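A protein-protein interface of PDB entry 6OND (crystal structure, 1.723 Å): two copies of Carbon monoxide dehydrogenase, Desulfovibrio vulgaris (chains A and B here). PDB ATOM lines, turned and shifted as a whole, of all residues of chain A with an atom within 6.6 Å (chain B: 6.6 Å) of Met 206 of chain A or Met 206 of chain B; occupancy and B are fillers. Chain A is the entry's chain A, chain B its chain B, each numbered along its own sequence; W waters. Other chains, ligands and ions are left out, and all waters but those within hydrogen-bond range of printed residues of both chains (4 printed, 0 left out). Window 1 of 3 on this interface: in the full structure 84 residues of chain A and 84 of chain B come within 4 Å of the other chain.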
ATOM      1  N   GLY A  95      25.457   3.248  -9.519  1.00  0.00           N
ATOM      2  CA  GLY A  95      25.851   4.467 -10.207  1.00  0.00           C
ATOM      3  C   GLY A  95      26.000   5.647  -9.266  1.00  0.00           C
ATOM      4  O   GLY A  95      26.959   6.420  -9.370  1.00  0.00           O
ATOM      5  N   ARG A  96      25.055   5.809  -8.335  1.00  0.00           N
ATOM      6  CA  ARG A  96      25.191   6.886  -7.353  1.00  0.00           C
ATOM      7  C   ARG A  96      26.381   6.662  -6.425  1.00  0.00           C
ATOM      8  O   ARG A  96      27.023   7.627  -6.007  1.00  0.00           O
ATOM      9  CB  ARG A  96      23.900   7.073  -6.548  1.00  0.00           C
ATOM     10  CG  ARG A  96      22.811   7.760  -7.319  1.00  0.00           C
ATOM     11  CD  ARG A  96      21.716   8.341  -6.420  1.00  0.00           C
ATOM     12  NE  ARG A  96      20.791   9.098  -7.253  1.00  0.00           N
ATOM     13  CZ  ARG A  96      19.720   9.748  -6.820  1.00  0.00           C
ATOM     14  NH1 ARG A  96      18.956  10.397  -7.698  1.00  0.00           N
ATOM     15  NH2 ARG A  96      19.411   9.751  -5.531  1.00  0.00           N
ATOM     16  N   PHE A  97      26.684   5.401  -6.102  1.00  0.00           N
ATOM     17  CA  PHE A  97      27.850   5.068  -5.287  1.00  0.00           C
ATOM     18  C   PHE A  97      29.144   5.513  -5.981  1.00  0.00           C
ATOM     19  O   PHE A  97      29.994   6.178  -5.374  1.00  0.00           O
ATOM     20  CB  PHE A  97      27.802   3.553  -5.049  1.00  0.00           C
ATOM     21  CG  PHE A  97      28.721   3.042  -3.977  1.00  0.00           C
ATOM     22  CD1 PHE A  97      28.278   2.909  -2.659  1.00  0.00           C
ATOM     23  CD2 PHE A  97      30.001   2.623  -4.302  1.00  0.00           C
ATOM     24  CE1 PHE A  97      29.130   2.409  -1.668  1.00  0.00           C
ATOM     25  CE2 PHE A  97      30.848   2.109  -3.328  1.00  0.00           C
ATOM     26  CZ  PHE A  97      30.414   2.010  -2.009  1.00  0.00           C
ATOM     27  N   ALA A  99      29.329   7.778  -8.378  1.00  0.00           N
ATOM     28  CA  ALA A  99      29.314   9.232  -8.515  1.00  0.00           C
ATOM     29  C   ALA A  99      29.814   9.913  -7.249  1.00  0.00           C
ATOM     30  O   ALA A  99      30.504  10.943  -7.324  1.00  0.00           O
ATOM     31  CB  ALA A  99      27.902   9.735  -8.843  1.00  0.00           C
ATOM     32  N   GLY A 100      29.476   9.363  -6.077  1.00  0.00           N
ATOM     33  CA  GLY A 100      29.996   9.928  -4.835  1.00  0.00           C
ATOM     34  C   GLY A 100      31.510   9.839  -4.757  1.00  0.00           C
ATOM     35  O   GLY A 100      32.176  10.738  -4.233  1.00  0.00           O
ATOM     36  N   GLY A 101      32.073   8.748  -5.268  1.00  0.00           N
ATOM     37  CA  GLY A 101      33.518   8.620  -5.275  1.00  0.00           C
ATOM     38  C   GLY A 101      34.157   9.593  -6.245  1.00  0.00           C
ATOM     39  O   GLY A 101      35.149  10.256  -5.919  1.00  0.00           O
ATOM     40  N   ALA A 103      32.960  12.375  -7.141  1.00  0.00           N
ATOM     41  CA  ALA A 103      32.793  13.729  -6.619  1.00  0.00           C
ATOM     42  C   ALA A 103      33.851  14.058  -5.578  1.00  0.00           C
ATOM     43  O   ALA A 103      34.302  15.204  -5.492  1.00  0.00           O
ATOM     44  CB  ALA A 103      31.388  13.924  -6.034  1.00  0.00           C
ATOM     45  N   GLY A 104      34.231  13.078  -4.759  1.00  0.00           N
ATOM     46  CA  GLY A 104      35.325  13.295  -3.823  1.00  0.00           C
ATOM     47  C   GLY A 104      36.619  13.694  -4.514  1.00  0.00           C
ATOM     48  O   GLY A 104      37.299  14.636  -4.102  1.00  0.00           O
ATOM     49  N   GLU A 201      29.484  14.901 -15.625  1.00  0.00           N
ATOM     50  CA  GLU A 201      29.131  13.482 -15.581  1.00  0.00           C
ATOM     51  C   GLU A 201      28.527  13.099 -14.241  1.00  0.00           C
ATOM     52  O   GLU A 201      27.650  12.236 -14.183  1.00  0.00           O
ATOM     53  CB  GLU A 201      30.333  12.577 -15.908  1.00  0.00           C
ATOM     54  CG  GLU A 201      31.133  12.936 -17.166  1.00  0.00           C
ATOM     55  CD  GLU A 201      30.312  13.037 -18.450  1.00  0.00           C
ATOM     56  OE1 GLU A 201      30.878  13.553 -19.436  1.00  0.00           O
ATOM     57  OE2 GLU A 201      29.133  12.605 -18.500  1.00  0.00           O
ATOM     58  N   ILE A 202      28.976  13.731 -13.150  1.00  0.00           N
ATOM     59  CA  ILE A 202      28.394  13.454 -11.842  1.00  0.00           C
ATOM     60  C   ILE A 202      26.951  13.937 -11.805  1.00  0.00           C
ATOM     61  O   ILE A 202      26.045  13.212 -11.380  1.00  0.00           O
ATOM     62  CB  ILE A 202      29.247  14.114 -10.736  1.00  0.00           C
ATOM     63  CG1 ILE A 202      30.621  13.444 -10.634  1.00  0.00           C
ATOM     64  CG2 ILE A 202      28.493  14.140  -9.383  1.00  0.00           C
ATOM     65  CD1 ILE A 202      31.673  14.360  -9.990  1.00  0.00           C
ATOM     66  N   ALA A 203      26.717  15.160 -12.277  1.00  0.00           N
ATOM     67  CA  ALA A 203      25.350  15.676 -12.357  1.00  0.00           C
ATOM     68  C   ALA A 203      24.478  14.791 -13.239  1.00  0.00           C
ATOM     69  O   ALA A 203      23.342  14.468 -12.877  1.00  0.00           O
ATOM     70  CB  ALA A 203      25.372  17.094 -12.918  1.00  0.00           C
ATOM     71  N   GLU A 204      24.996  14.380 -14.399  1.00  0.00           N
ATOM     72  CA  GLU A 204      24.208  13.520 -15.270  1.00  0.00           C
ATOM     73  C   GLU A 204      23.870  12.190 -14.603  1.00  0.00           C
ATOM     74  O   GLU A 204      22.787  11.635 -14.828  1.00  0.00           O
ATOM     75  CB  GLU A 204      24.884  13.305 -16.626  1.00  0.00           C
ATOM     76  CG  GLU A 204      24.034  12.382 -17.506  1.00  0.00           C
ATOM     77  CD  GLU A 204      24.515  12.237 -18.945  1.00  0.00           C
ATOM     78  OE1 GLU A 204      24.443  11.101 -19.459  1.00  0.00           O
ATOM     79  OE2 GLU A 204      24.917  13.246 -19.575  1.00  0.00           O
ATOM     80  N   MET A 205      24.785  11.645 -13.799  1.00  0.00           N
ATOM     81  CA  MET A 205      24.473  10.410 -13.086  1.00  0.00           C
ATOM     82  C   MET A 205      23.335  10.608 -12.093  1.00  0.00           C
ATOM     83  O   MET A 205      22.478   9.730 -11.933  1.00  0.00           O
ATOM     84  CB  MET A 205      25.702   9.866 -12.360  1.00  0.00           C
ATOM     85  CG  MET A 205      25.408   8.596 -11.552  1.00  0.00           C
ATOM     86  SD  MET A 205      24.874   7.195 -12.594  1.00  0.00           S
ATOM     87  CE  MET A 205      26.487   6.644 -13.080  1.00  0.00           C
ATOM     88  N   MET A 206      23.329  11.738 -11.392  1.00  0.00           N
ATOM     89  CA  MET A 206      22.256  11.980 -10.437  1.00  0.00           C
ATOM     90  C   MET A 206      20.910  12.170 -11.130  1.00  0.00           C
ATOM     91  O   MET A 206      19.882  11.768 -10.581  1.00  0.00           O
ATOM     92  CB  MET A 206      22.614  13.166  -9.537  1.00  0.00           C
ATOM     93  CG  MET A 206      23.829  12.917  -8.646  1.00  0.00           C
ATOM     94  SD  MET A 206      23.615  11.472  -7.565  1.00  0.00           S
ATOM     95  CE  MET A 206      22.320  12.102  -6.477  1.00  0.00           C
ATOM     96  N   HIS A 207      20.896  12.772 -12.324  1.00  0.00           N
ATOM     97  CA  HIS A 207      19.682  12.860 -13.129  1.00  0.00           C
ATOM     98  C   HIS A 207      19.233  11.482 -13.598  1.00  0.00           C
ATOM     99  O   HIS A 207      18.051  11.126 -13.484  1.00  0.00           O
ATOM    100  CB  HIS A 207      19.949  13.769 -14.331  1.00  0.00           C
ATOM    101  CG  HIS A 207      18.845  13.797 -15.344  1.00  0.00           C
ATOM    102  ND1 HIS A 207      19.075  14.041 -16.681  1.00  0.00           N
ATOM    103  CD2 HIS A 207      17.506  13.635 -15.218  1.00  0.00           C
ATOM    104  CE1 HIS A 207      17.929  14.023 -17.339  1.00  0.00           C
ATOM    105  NE2 HIS A 207      16.962  13.776 -16.474  1.00  0.00           N
ATOM    106  N   ARG A 208      20.171  10.686 -14.131  1.00  0.00           N
ATOM    107  CA  ARG A 208      19.792   9.378 -14.664  1.00  0.00           C
ATOM    108  C   ARG A 208      19.158   8.507 -13.591  1.00  0.00           C
ATOM    109  O   ARG A 208      18.299   7.675 -13.896  1.00  0.00           O
ATOM    110  CB  ARG A 208      21.022   8.661 -15.243  1.00  0.00           C
ATOM    111  CG  ARG A 208      21.431   9.120 -16.636  1.00  0.00           C
ATOM    112  CD  ARG A 208      22.643   8.347 -17.157  1.00  0.00           C
ATOM    113  NE  ARG A 208      23.090   8.903 -18.440  1.00  0.00           N
ATOM    114  CZ  ARG A 208      22.831   8.358 -19.620  1.00  0.00           C
ATOM    115  NH1 ARG A 208      22.147   7.225 -19.688  1.00  0.00           N
ATOM    116  NH2 ARG A 208      23.252   8.948 -20.738  1.00  0.00           N
ATOM    117  N   THR A 209      19.548   8.693 -12.332  1.00  0.00           N
ATOM    118  CA  THR A 209      19.102   7.799 -11.273  1.00  0.00           C
ATOM    119  C   THR A 209      17.839   8.277 -10.553  1.00  0.00           C
ATOM    120  O   THR A 209      17.347   7.564  -9.675  1.00  0.00           O
ATOM    121  CB  THR A 209      20.235   7.515 -10.283  1.00  0.00           C
ATOM    122  OG1 THR A 209      20.775   8.757  -9.797  1.00  0.00           O
ATOM    123  CG2 THR A 209      21.352   6.706 -10.960  1.00  0.00           C
ATOM    124  N   HIS A 210      17.315   9.453 -10.907  1.00  0.00           N
ATOM    125  CA  HIS A 210      15.989   9.901 -10.470  1.00  0.00           C
ATOM    126  C   HIS A 210      14.921   8.942 -11.003  1.00  0.00           C
ATOM    127  O   HIS A 210      15.093   8.318 -12.058  1.00  0.00           O
ATOM    128  CB  HIS A 210      15.759  11.311 -11.050  1.00  0.00           C
ATOM    129  CG  HIS A 210      14.554  12.031 -10.517  1.00  0.00           C
ATOM    130  ND1 HIS A 210      13.274  11.745 -10.931  1.00  0.00           N
ATOM    131  CD2 HIS A 210      14.442  13.066  -9.646  1.00  0.00           C
ATOM    132  CE1 HIS A 210      12.418  12.540 -10.311  1.00  0.00           C
ATOM    133  NE2 HIS A 210      13.101  13.354  -9.525  1.00  0.00           N
ATOM    134  N   HIS A 223      27.202   4.699 -18.186  1.00  0.00           N
ATOM    135  CA  HIS A 223      27.436   6.044 -17.674  1.00  0.00           C
ATOM    136  C   HIS A 223      28.278   6.031 -16.400  1.00  0.00           C
ATOM    137  O   HIS A 223      29.049   6.969 -16.167  1.00  0.00           O
ATOM    138  CB  HIS A 223      26.150   6.863 -17.490  1.00  0.00           C
ATOM    139  CG  HIS A 223      26.434   8.280 -17.091  1.00  0.00           C
ATOM    140  ND1 HIS A 223      27.056   9.172 -17.939  1.00  0.00           N
ATOM    141  CD2 HIS A 223      26.288   8.928 -15.907  1.00  0.00           C
ATOM    142  CE1 HIS A 223      27.247  10.321 -17.308  1.00  0.00           C
ATOM    143  NE2 HIS A 223      26.801  10.195 -16.069  1.00  0.00           N
ATOM    144  N   GLU A 563      33.466   4.823  -1.437  1.00  0.00           N
ATOM    145  CA  GLU A 563      32.986   5.139  -2.778  1.00  0.00           C
ATOM    146  C   GLU A 563      34.142   5.552  -3.681  1.00  0.00           C
ATOM    147  O   GLU A 563      34.144   5.246  -4.880  1.00  0.00           O
ATOM    148  CB  GLU A 563      31.935   6.254  -2.707  1.00  0.00           C
ATOM    149  CG  GLU A 563      30.583   5.774  -2.197  1.00  0.00           C
ATOM    150  CD  GLU A 563      29.554   6.895  -1.978  1.00  0.00           C
ATOM    151  OE1 GLU A 563      29.949   8.013  -1.580  1.00  0.00           O
ATOM    152  OE2 GLU A 563      28.340   6.644  -2.176  1.00  0.00           O
ATOM    153  N   GLY B  95      20.287  15.339   1.808  1.00  0.00           N
ATOM    154  CA  GLY B  95      21.103  16.119   0.891  1.00  0.00           C
ATOM    155  C   GLY B  95      21.223  15.479  -0.480  1.00  0.00           C
ATOM    156  O   GLY B  95      21.101  16.156  -1.506  1.00  0.00           O
ATOM    157  N   ARG B  96      21.495  14.167  -0.524  1.00  0.00           N
ATOM    158  CA  ARG B  96      21.567  13.494  -1.825  1.00  0.00           C
ATOM    159  C   ARG B  96      20.203  13.471  -2.498  1.00  0.00           C
ATOM    160  O   ARG B  96      20.106  13.566  -3.730  1.00  0.00           O
ATOM    161  CB  ARG B  96      22.140  12.079  -1.701  1.00  0.00           C
ATOM    162  CG  ARG B  96      23.638  12.054  -1.407  1.00  0.00           C
ATOM    163  CD  ARG B  96      24.301  10.686  -1.634  1.00  0.00           C
ATOM    164  NE  ARG B  96      25.751  10.849  -1.510  1.00  0.00           N
ATOM    165  CZ  ARG B  96      26.652   9.885  -1.685  1.00  0.00           C
ATOM    166  NH1 ARG B  96      27.949  10.173  -1.559  1.00  0.00           N
ATOM    167  NH2 ARG B  96      26.269   8.641  -1.990  1.00  0.00           N
ATOM    168  N   PHE B  97      19.142  13.317  -1.704  1.00  0.00           N
ATOM    169  CA  PHE B  97      17.788  13.392  -2.245  1.00  0.00           C
ATOM    170  C   PHE B  97      17.585  14.706  -2.992  1.00  0.00           C
ATOM    171  O   PHE B  97      17.156  14.720  -4.154  1.00  0.00           O
ATOM    172  CB  PHE B  97      16.805  13.252  -1.086  1.00  0.00           C
ATOM    173  CG  PHE B  97      15.401  12.899  -1.497  1.00  0.00           C
ATOM    174  CD1 PHE B  97      15.022  11.574  -1.666  1.00  0.00           C
ATOM    175  CD2 PHE B  97      14.449  13.898  -1.663  1.00  0.00           C
ATOM    176  CE1 PHE B  97      13.729  11.245  -2.015  1.00  0.00           C
ATOM    177  CE2 PHE B  97      13.139  13.579  -2.013  1.00  0.00           C
ATOM    178  CZ  PHE B  97      12.778  12.253  -2.191  1.00  0.00           C
ATOM    179  N   ALA B  99      19.893  16.709  -4.115  1.00  0.00           N
ATOM    180  CA  ALA B  99      20.822  16.824  -5.237  1.00  0.00           C
ATOM    181  C   ALA B  99      20.282  16.119  -6.475  1.00  0.00           C
ATOM    182  O   ALA B  99      20.465  16.603  -7.596  1.00  0.00           O
ATOM    183  CB  ALA B  99      22.205  16.279  -4.861  1.00  0.00           C
ATOM    184  N   GLY B 100      19.620  14.972  -6.293  1.00  0.00           N
ATOM    185  CA  GLY B 100      19.041  14.281  -7.440  1.00  0.00           C
ATOM    186  C   GLY B 100      17.943  15.087  -8.109  1.00  0.00           C
ATOM    187  O   GLY B 100      17.804  15.068  -9.337  1.00  0.00           O
ATOM    188  N   GLY B 101      17.143  15.800  -7.312  1.00  0.00           N
ATOM    189  CA  GLY B 101      16.118  16.652  -7.888  1.00  0.00           C
ATOM    190  C   GLY B 101      16.712  17.834  -8.625  1.00  0.00           C
ATOM    191  O   GLY B 101      16.281  18.170  -9.731  1.00  0.00           O
ATOM    192  N   ALA B 103      19.569  17.929 -10.011  1.00  0.00           N
ATOM    193  CA  ALA B 103      20.211  17.398 -11.216  1.00  0.00           C
ATOM    194  C   ALA B 103      19.213  17.198 -12.350  1.00  0.00           C
ATOM    195  O   ALA B 103      19.553  17.389 -13.523  1.00  0.00           O
ATOM    196  CB  ALA B 103      20.910  16.078 -10.893  1.00  0.00           C
ATOM    197  N   GLY B 104      17.991  16.773 -12.023  1.00  0.00           N
ATOM    198  CA  GLY B 104      16.961  16.652 -13.047  1.00  0.00           C
ATOM    199  C   GLY B 104      16.697  17.969 -13.756  1.00  0.00           C
ATOM    200  O   GLY B 104      16.718  18.047 -14.986  1.00  0.00           O
ATOM    201  N   GLU B 201      27.306  22.759  -7.542  1.00  0.00           N
ATOM    202  CA  GLU B 201      26.671  22.522  -6.243  1.00  0.00           C
ATOM    203  C   GLU B 201      26.230  21.076  -6.101  1.00  0.00           C
ATOM    204  O   GLU B 201      26.272  20.524  -4.997  1.00  0.00           O
ATOM    205  CB  GLU B 201      25.488  23.466  -5.977  1.00  0.00           C
ATOM    206  CG  GLU B 201      25.770  24.975  -6.156  1.00  0.00           C
ATOM    207  CD  GLU B 201      26.999  25.509  -5.417  1.00  0.00           C
ATOM    208  OE1 GLU B 201      27.439  26.630  -5.765  1.00  0.00           O
ATOM    209  OE2 GLU B 201      27.529  24.850  -4.491  1.00  0.00           O
ATOM    210  N   ILE B 202      25.809  20.443  -7.202  1.00  0.00           N
ATOM    211  CA  ILE B 202      25.461  19.027  -7.151  1.00  0.00           C
ATOM    212  C   ILE B 202      26.688  18.178  -6.823  1.00  0.00           C
ATOM    213  O   ILE B 202      26.641  17.287  -5.964  1.00  0.00           O
ATOM    214  CB  ILE B 202      24.801  18.601  -8.471  1.00  0.00           C
ATOM    215  CG1 ILE B 202      23.496  19.380  -8.662  1.00  0.00           C
ATOM    216  CG2 ILE B 202      24.569  17.087  -8.485  1.00  0.00           C
ATOM    217  CD1 ILE B 202      22.912  19.278 -10.098  1.00  0.00           C
ATOM    218  N   ALA B 203      27.799  18.419  -7.526  1.00  0.00           N
ATOM    219  CA  ALA B 203      29.012  17.653  -7.254  1.00  0.00           C
ATOM    220  C   ALA B 203      29.477  17.851  -5.814  1.00  0.00           C
ATOM    221  O   ALA B 203      29.908  16.900  -5.154  1.00  0.00           O
ATOM    222  CB  ALA B 203      30.116  18.058  -8.229  1.00  0.00           C
ATOM    223  N   GLU B 204      29.380  19.077  -5.299  1.00  0.00           N
ATOM    224  CA  GLU B 204      29.823  19.297  -3.924  1.00  0.00           C
ATOM    225  C   GLU B 204      28.931  18.568  -2.926  1.00  0.00           C
ATOM    226  O   GLU B 204      29.426  18.041  -1.919  1.00  0.00           O
ATOM    227  CB  GLU B 204      29.929  20.789  -3.597  1.00  0.00           C
ATOM    228  CG  GLU B 204      30.341  21.001  -2.131  1.00  0.00           C
ATOM    229  CD  GLU B 204      30.664  22.431  -1.771  1.00  0.00           C
ATOM    230  OE1 GLU B 204      31.312  23.133  -2.567  1.00  0.00           O
ATOM    231  OE2 GLU B 204      30.268  22.852  -0.666  1.00  0.00           O
ATOM    232  N   MET B 205      27.617  18.499  -3.195  1.00  0.00           N
ATOM    233  CA  MET B 205      26.748  17.708  -2.321  1.00  0.00           C
ATOM    234  C   MET B 205      27.174  16.247  -2.295  1.00  0.00           C
ATOM    235  O   MET B 205      27.161  15.604  -1.238  1.00  0.00           O
ATOM    236  CB  MET B 205      25.279  17.817  -2.739  1.00  0.00           C
ATOM    237  CG  MET B 205      24.349  17.019  -1.798  1.00  0.00           C
ATOM    238  SD  MET B 205      24.464  17.600  -0.077  1.00  0.00           S
ATOM    239  CE  MET B 205      23.258  18.868  -0.200  1.00  0.00           C
ATOM    240  N   MET B 206      27.526  15.693  -3.453  1.00  0.00           N
ATOM    241  CA  MET B 206      27.946  14.301  -3.477  1.00  0.00           C
ATOM    242  C   MET B 206      29.274  14.109  -2.754  1.00  0.00           C
ATOM    243  O   MET B 206      29.482  13.071  -2.122  1.00  0.00           O
ATOM    244  CB  MET B 206      27.985  13.790  -4.920  1.00  0.00           C
ATOM    245  CG  MET B 206      26.593  13.804  -5.566  1.00  0.00           C
ATOM    246  SD  MET B 206      25.425  12.752  -4.664  1.00  0.00           S
ATOM    247  CE  MET B 206      26.143  11.132  -4.970  1.00  0.00           C
ATOM    248  N   HIS B 207      30.165  15.099  -2.814  1.00  0.00           N
ATOM    249  CA  HIS B 207      31.406  15.033  -2.041  1.00  0.00           C
ATOM    250  C   HIS B 207      31.116  15.092  -0.544  1.00  0.00           C
ATOM    251  O   HIS B 207      31.591  14.248   0.232  1.00  0.00           O
ATOM    252  CB  HIS B 207      32.328  16.177  -2.486  1.00  0.00           C
ATOM    253  CG  HIS B 207      33.536  16.369  -1.620  1.00  0.00           C
ATOM    254  ND1 HIS B 207      34.128  17.600  -1.446  1.00  0.00           N
ATOM    255  CD2 HIS B 207      34.275  15.490  -0.900  1.00  0.00           C
ATOM    256  CE1 HIS B 207      35.175  17.475  -0.647  1.00  0.00           C
ATOM    257  NE2 HIS B 207      35.285  16.205  -0.302  1.00  0.00           N
ATOM    258  N   ARG B 208      30.285  16.049  -0.125  1.00  0.00           N
ATOM    259  CA  ARG B 208      30.034  16.261   1.304  1.00  0.00           C
ATOM    260  C   ARG B 208      29.433  15.035   1.978  1.00  0.00           C
ATOM    261  O   ARG B 208      29.661  14.815   3.175  1.00  0.00           O
ATOM    262  CB  ARG B 208      29.077  17.435   1.497  1.00  0.00           C
ATOM    263  CG  ARG B 208      29.749  18.797   1.412  1.00  0.00           C
ATOM    264  CD  ARG B 208      28.748  19.907   1.696  1.00  0.00           C
ATOM    265  NE  ARG B 208      29.332  21.200   1.406  1.00  0.00           N
ATOM    266  CZ  ARG B 208      29.747  22.044   2.336  1.00  0.00           C
ATOM    267  NH1 ARG B 208      30.293  23.200   1.987  1.00  0.00           N
ATOM    268  NH2 ARG B 208      29.618  21.721   3.612  1.00  0.00           N
ATOM    269  N   THR B 209      28.690  14.221   1.228  1.00  0.00           N
ATOM    270  CA  THR B 209      27.954  13.086   1.765  1.00  0.00           C
ATOM    271  C   THR B 209      28.729  11.772   1.721  1.00  0.00           C
ATOM    272  O   THR B 209      28.203  10.756   2.185  1.00  0.00           O
ATOM    273  CB  THR B 209      26.599  12.950   1.058  1.00  0.00           C
ATOM    274  OG1 THR B 209      26.784  12.943  -0.370  1.00  0.00           O
ATOM    275  CG2 THR B 209      25.684  14.114   1.425  1.00  0.00           C
ATOM    276  N   HIS B 210      29.947  11.773   1.174  1.00  0.00           N
ATOM    277  CA  HIS B 210      30.859  10.633   1.261  1.00  0.00           C
ATOM    278  C   HIS B 210      31.254  10.420   2.721  1.00  0.00           C
ATOM    279  O   HIS B 210      31.239  11.355   3.528  1.00  0.00           O
ATOM    280  CB  HIS B 210      32.100  10.948   0.403  1.00  0.00           C
ATOM    281  CG  HIS B 210      33.062   9.809   0.240  1.00  0.00           C
ATOM    282  ND1 HIS B 210      33.905   9.386   1.249  1.00  0.00           N
ATOM    283  CD2 HIS B 210      33.354   9.040  -0.841  1.00  0.00           C
ATOM    284  CE1 HIS B 210      34.649   8.387   0.809  1.00  0.00           C
ATOM    285  NE2 HIS B 210      34.337   8.159  -0.457  1.00  0.00           N
ATOM    286  N   HIS B 223      24.117  23.423   2.755  1.00  0.00           N
ATOM    287  CA  HIS B 223      24.505  23.154   1.376  1.00  0.00           C
ATOM    288  C   HIS B 223      23.346  22.590   0.564  1.00  0.00           C
ATOM    289  O   HIS B 223      23.297  22.780  -0.657  1.00  0.00           O
ATOM    290  CB  HIS B 223      25.732  22.246   1.253  1.00  0.00           C
ATOM    291  CG  HIS B 223      26.161  22.082  -0.164  1.00  0.00           C
ATOM    292  ND1 HIS B 223      26.634  23.136  -0.913  1.00  0.00           N
ATOM    293  CD2 HIS B 223      26.069  21.027  -1.010  1.00  0.00           C
ATOM    294  CE1 HIS B 223      26.868  22.726  -2.149  1.00  0.00           C
ATOM    295  NE2 HIS B 223      26.535  21.450  -2.233  1.00  0.00           N
ATOM    296  N   GLU B 563      12.155  13.605  -6.077  1.00  0.00           N
ATOM    297  CA  GLU B 563      13.289  14.429  -5.649  1.00  0.00           C
ATOM    298  C   GLU B 563      13.178  15.845  -6.204  1.00  0.00           C
ATOM    299  O   GLU B 563      13.539  16.809  -5.522  1.00  0.00           O
ATOM    300  CB  GLU B 563      14.623  13.770  -6.063  1.00  0.00           C
ATOM    301  CG  GLU B 563      14.911  12.437  -5.332  1.00  0.00           C
ATOM    302  CD  GLU B 563      16.183  11.689  -5.825  1.00  0.00           C
ATOM    303  OE1 GLU B 563      16.383  11.554  -7.054  1.00  0.00           O
ATOM    304  OE2 GLU B 563      16.968  11.195  -4.979  1.00  0.00           O
HETATM  305  O   HOH W   1      17.577   9.473  -2.591  1.00  0.00           O
HETATM  306  O   HOH W   2      25.798   5.227  -1.943  1.00  0.00           O
HETATM  307  O   HOH W   3      31.464   7.329   0.926  1.00  0.00           O
HETATM  308  O   HOH W   4      13.461  10.646  -7.761  1.00  0.00           O
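The side-chain carboxylate of Glu 563 of chain B lies within salt-bridge range of the guanidinium group of Arg 96 of chain A (2.9 Å).
The side-chain carboxylate (OE2) of Glu 563 of chain A lies within salt-bridge range of the guanidinium group (NH2) of Arg 96 of chain B (2.9 Å).
The side-chain sulfur (SD) of Met 206 of chain B lies close to the side-chain sulfur (SD) of Met 206 of chain A (3.7 Å).
The guanidinium group (NH1) of Arg 96 of chain A is in hydrogen-bond range of the backbone carbonyl oxygen (O) of Met 206 of chain A (3.3 Å).
NE of Arg 96 of chain A is in hydrogen-bond range of OG1 of Thr 209 of chain A, at 2.6 Å.
The guanidinium group (NE) of Arg 96 of chain B is in hydrogen-bond range of the side-chain hydroxyl (OG1) of Thr 209 of chain B (2.6 Å).
O of Arg 96 of chain A touches CE of Met 206 of chain B, 3.8 Å away.
Gly 100 of chain A touches His 210 of chain B.
His 207 of chain B touches Gly 104 of chain A.
Ala 103 of chain B touches Ala 203 of chain A (CB to O, 3.5 Å).
Met 206 of chain A touches Ala 103 of chain B.
His 210 of chain A touches Gly 100 of chain B.
OE1 of Glu 563 of chain B touches CD2 of His 210 of chain A, at 3.6 Å.
Of chain B, only Arg 96, Gly 100, Ala 103 and Met 206 come within 4 Å of Met 206 of chain A.
Met 206 of chain B touches just these residues of chain A: Arg 96 (3.8 Å), Gly 100 (3.9 Å), Ala 103 (3.6 Å) and Met 206 (3.6 Å).
Printed residues of chain A within 4 Å of Ala 203 of chain B: Ala 103 (3.4 Å).
Printed residues of chain B within 4 Å of Glu 563 of chain A: Arg 96 and His 210.
Printed residues of chain B within 4 Å of His 210 of chain A: Gly 100 and Glu 563.
Thr 209 of chain B touches none of the printed residues of chain A.
Of the 20 printed residues of chain B, 9 touch a printed residue of chain A.
Of the 20 printed residues of chain A, 9 touch a printed residue of chain B.
Hydrophobic or aromatic side chains of chain A within 4 Å of the printed part of chain B: Ala 103, Met 206, His 207 and His 210.
Among the printed residues, 21 pairs touch across the chains.
Among the printed residues, Asp or Glu carboxylates within 4 Å of a Lys or Arg side-chain nitrogen of the other chain: Arg 96 of chain A with Glu 563 of chain B and Glu 563 of chain A with Arg 96 of chain B.
Arg 96 of chain A touches Glu 563 of chain B, and with the chains exchanged Glu 563 of chain A touches Arg 96 of chain B.
Gly 104 of chain A touches His 207 of chain B, and with the chains exchanged His 207 of chain A touches Gly 104 of chain B.
Of the 21 pairs that touch across the chains among the printed residues, 21 have their exchanged pair printed and touching as well.
Water W2 lies within hydrogen-bond range of OE2 of Glu 563 of chain A (2.9 Å) and NH2 of Arg 96 of chain B (3.4 Å).
Water W1 bridges the side-chain carboxylate (OE2) of Glu 563 of chain B (3.0 Å) and the guanidinium group (NH2) of Arg 96 of chain A (3.5 Å).
Water W4 lies within hydrogen-bond range of OE1 of Glu 563 of chain B (3.1 Å) and NE2 of His 210 of chain A (3.3 Å).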
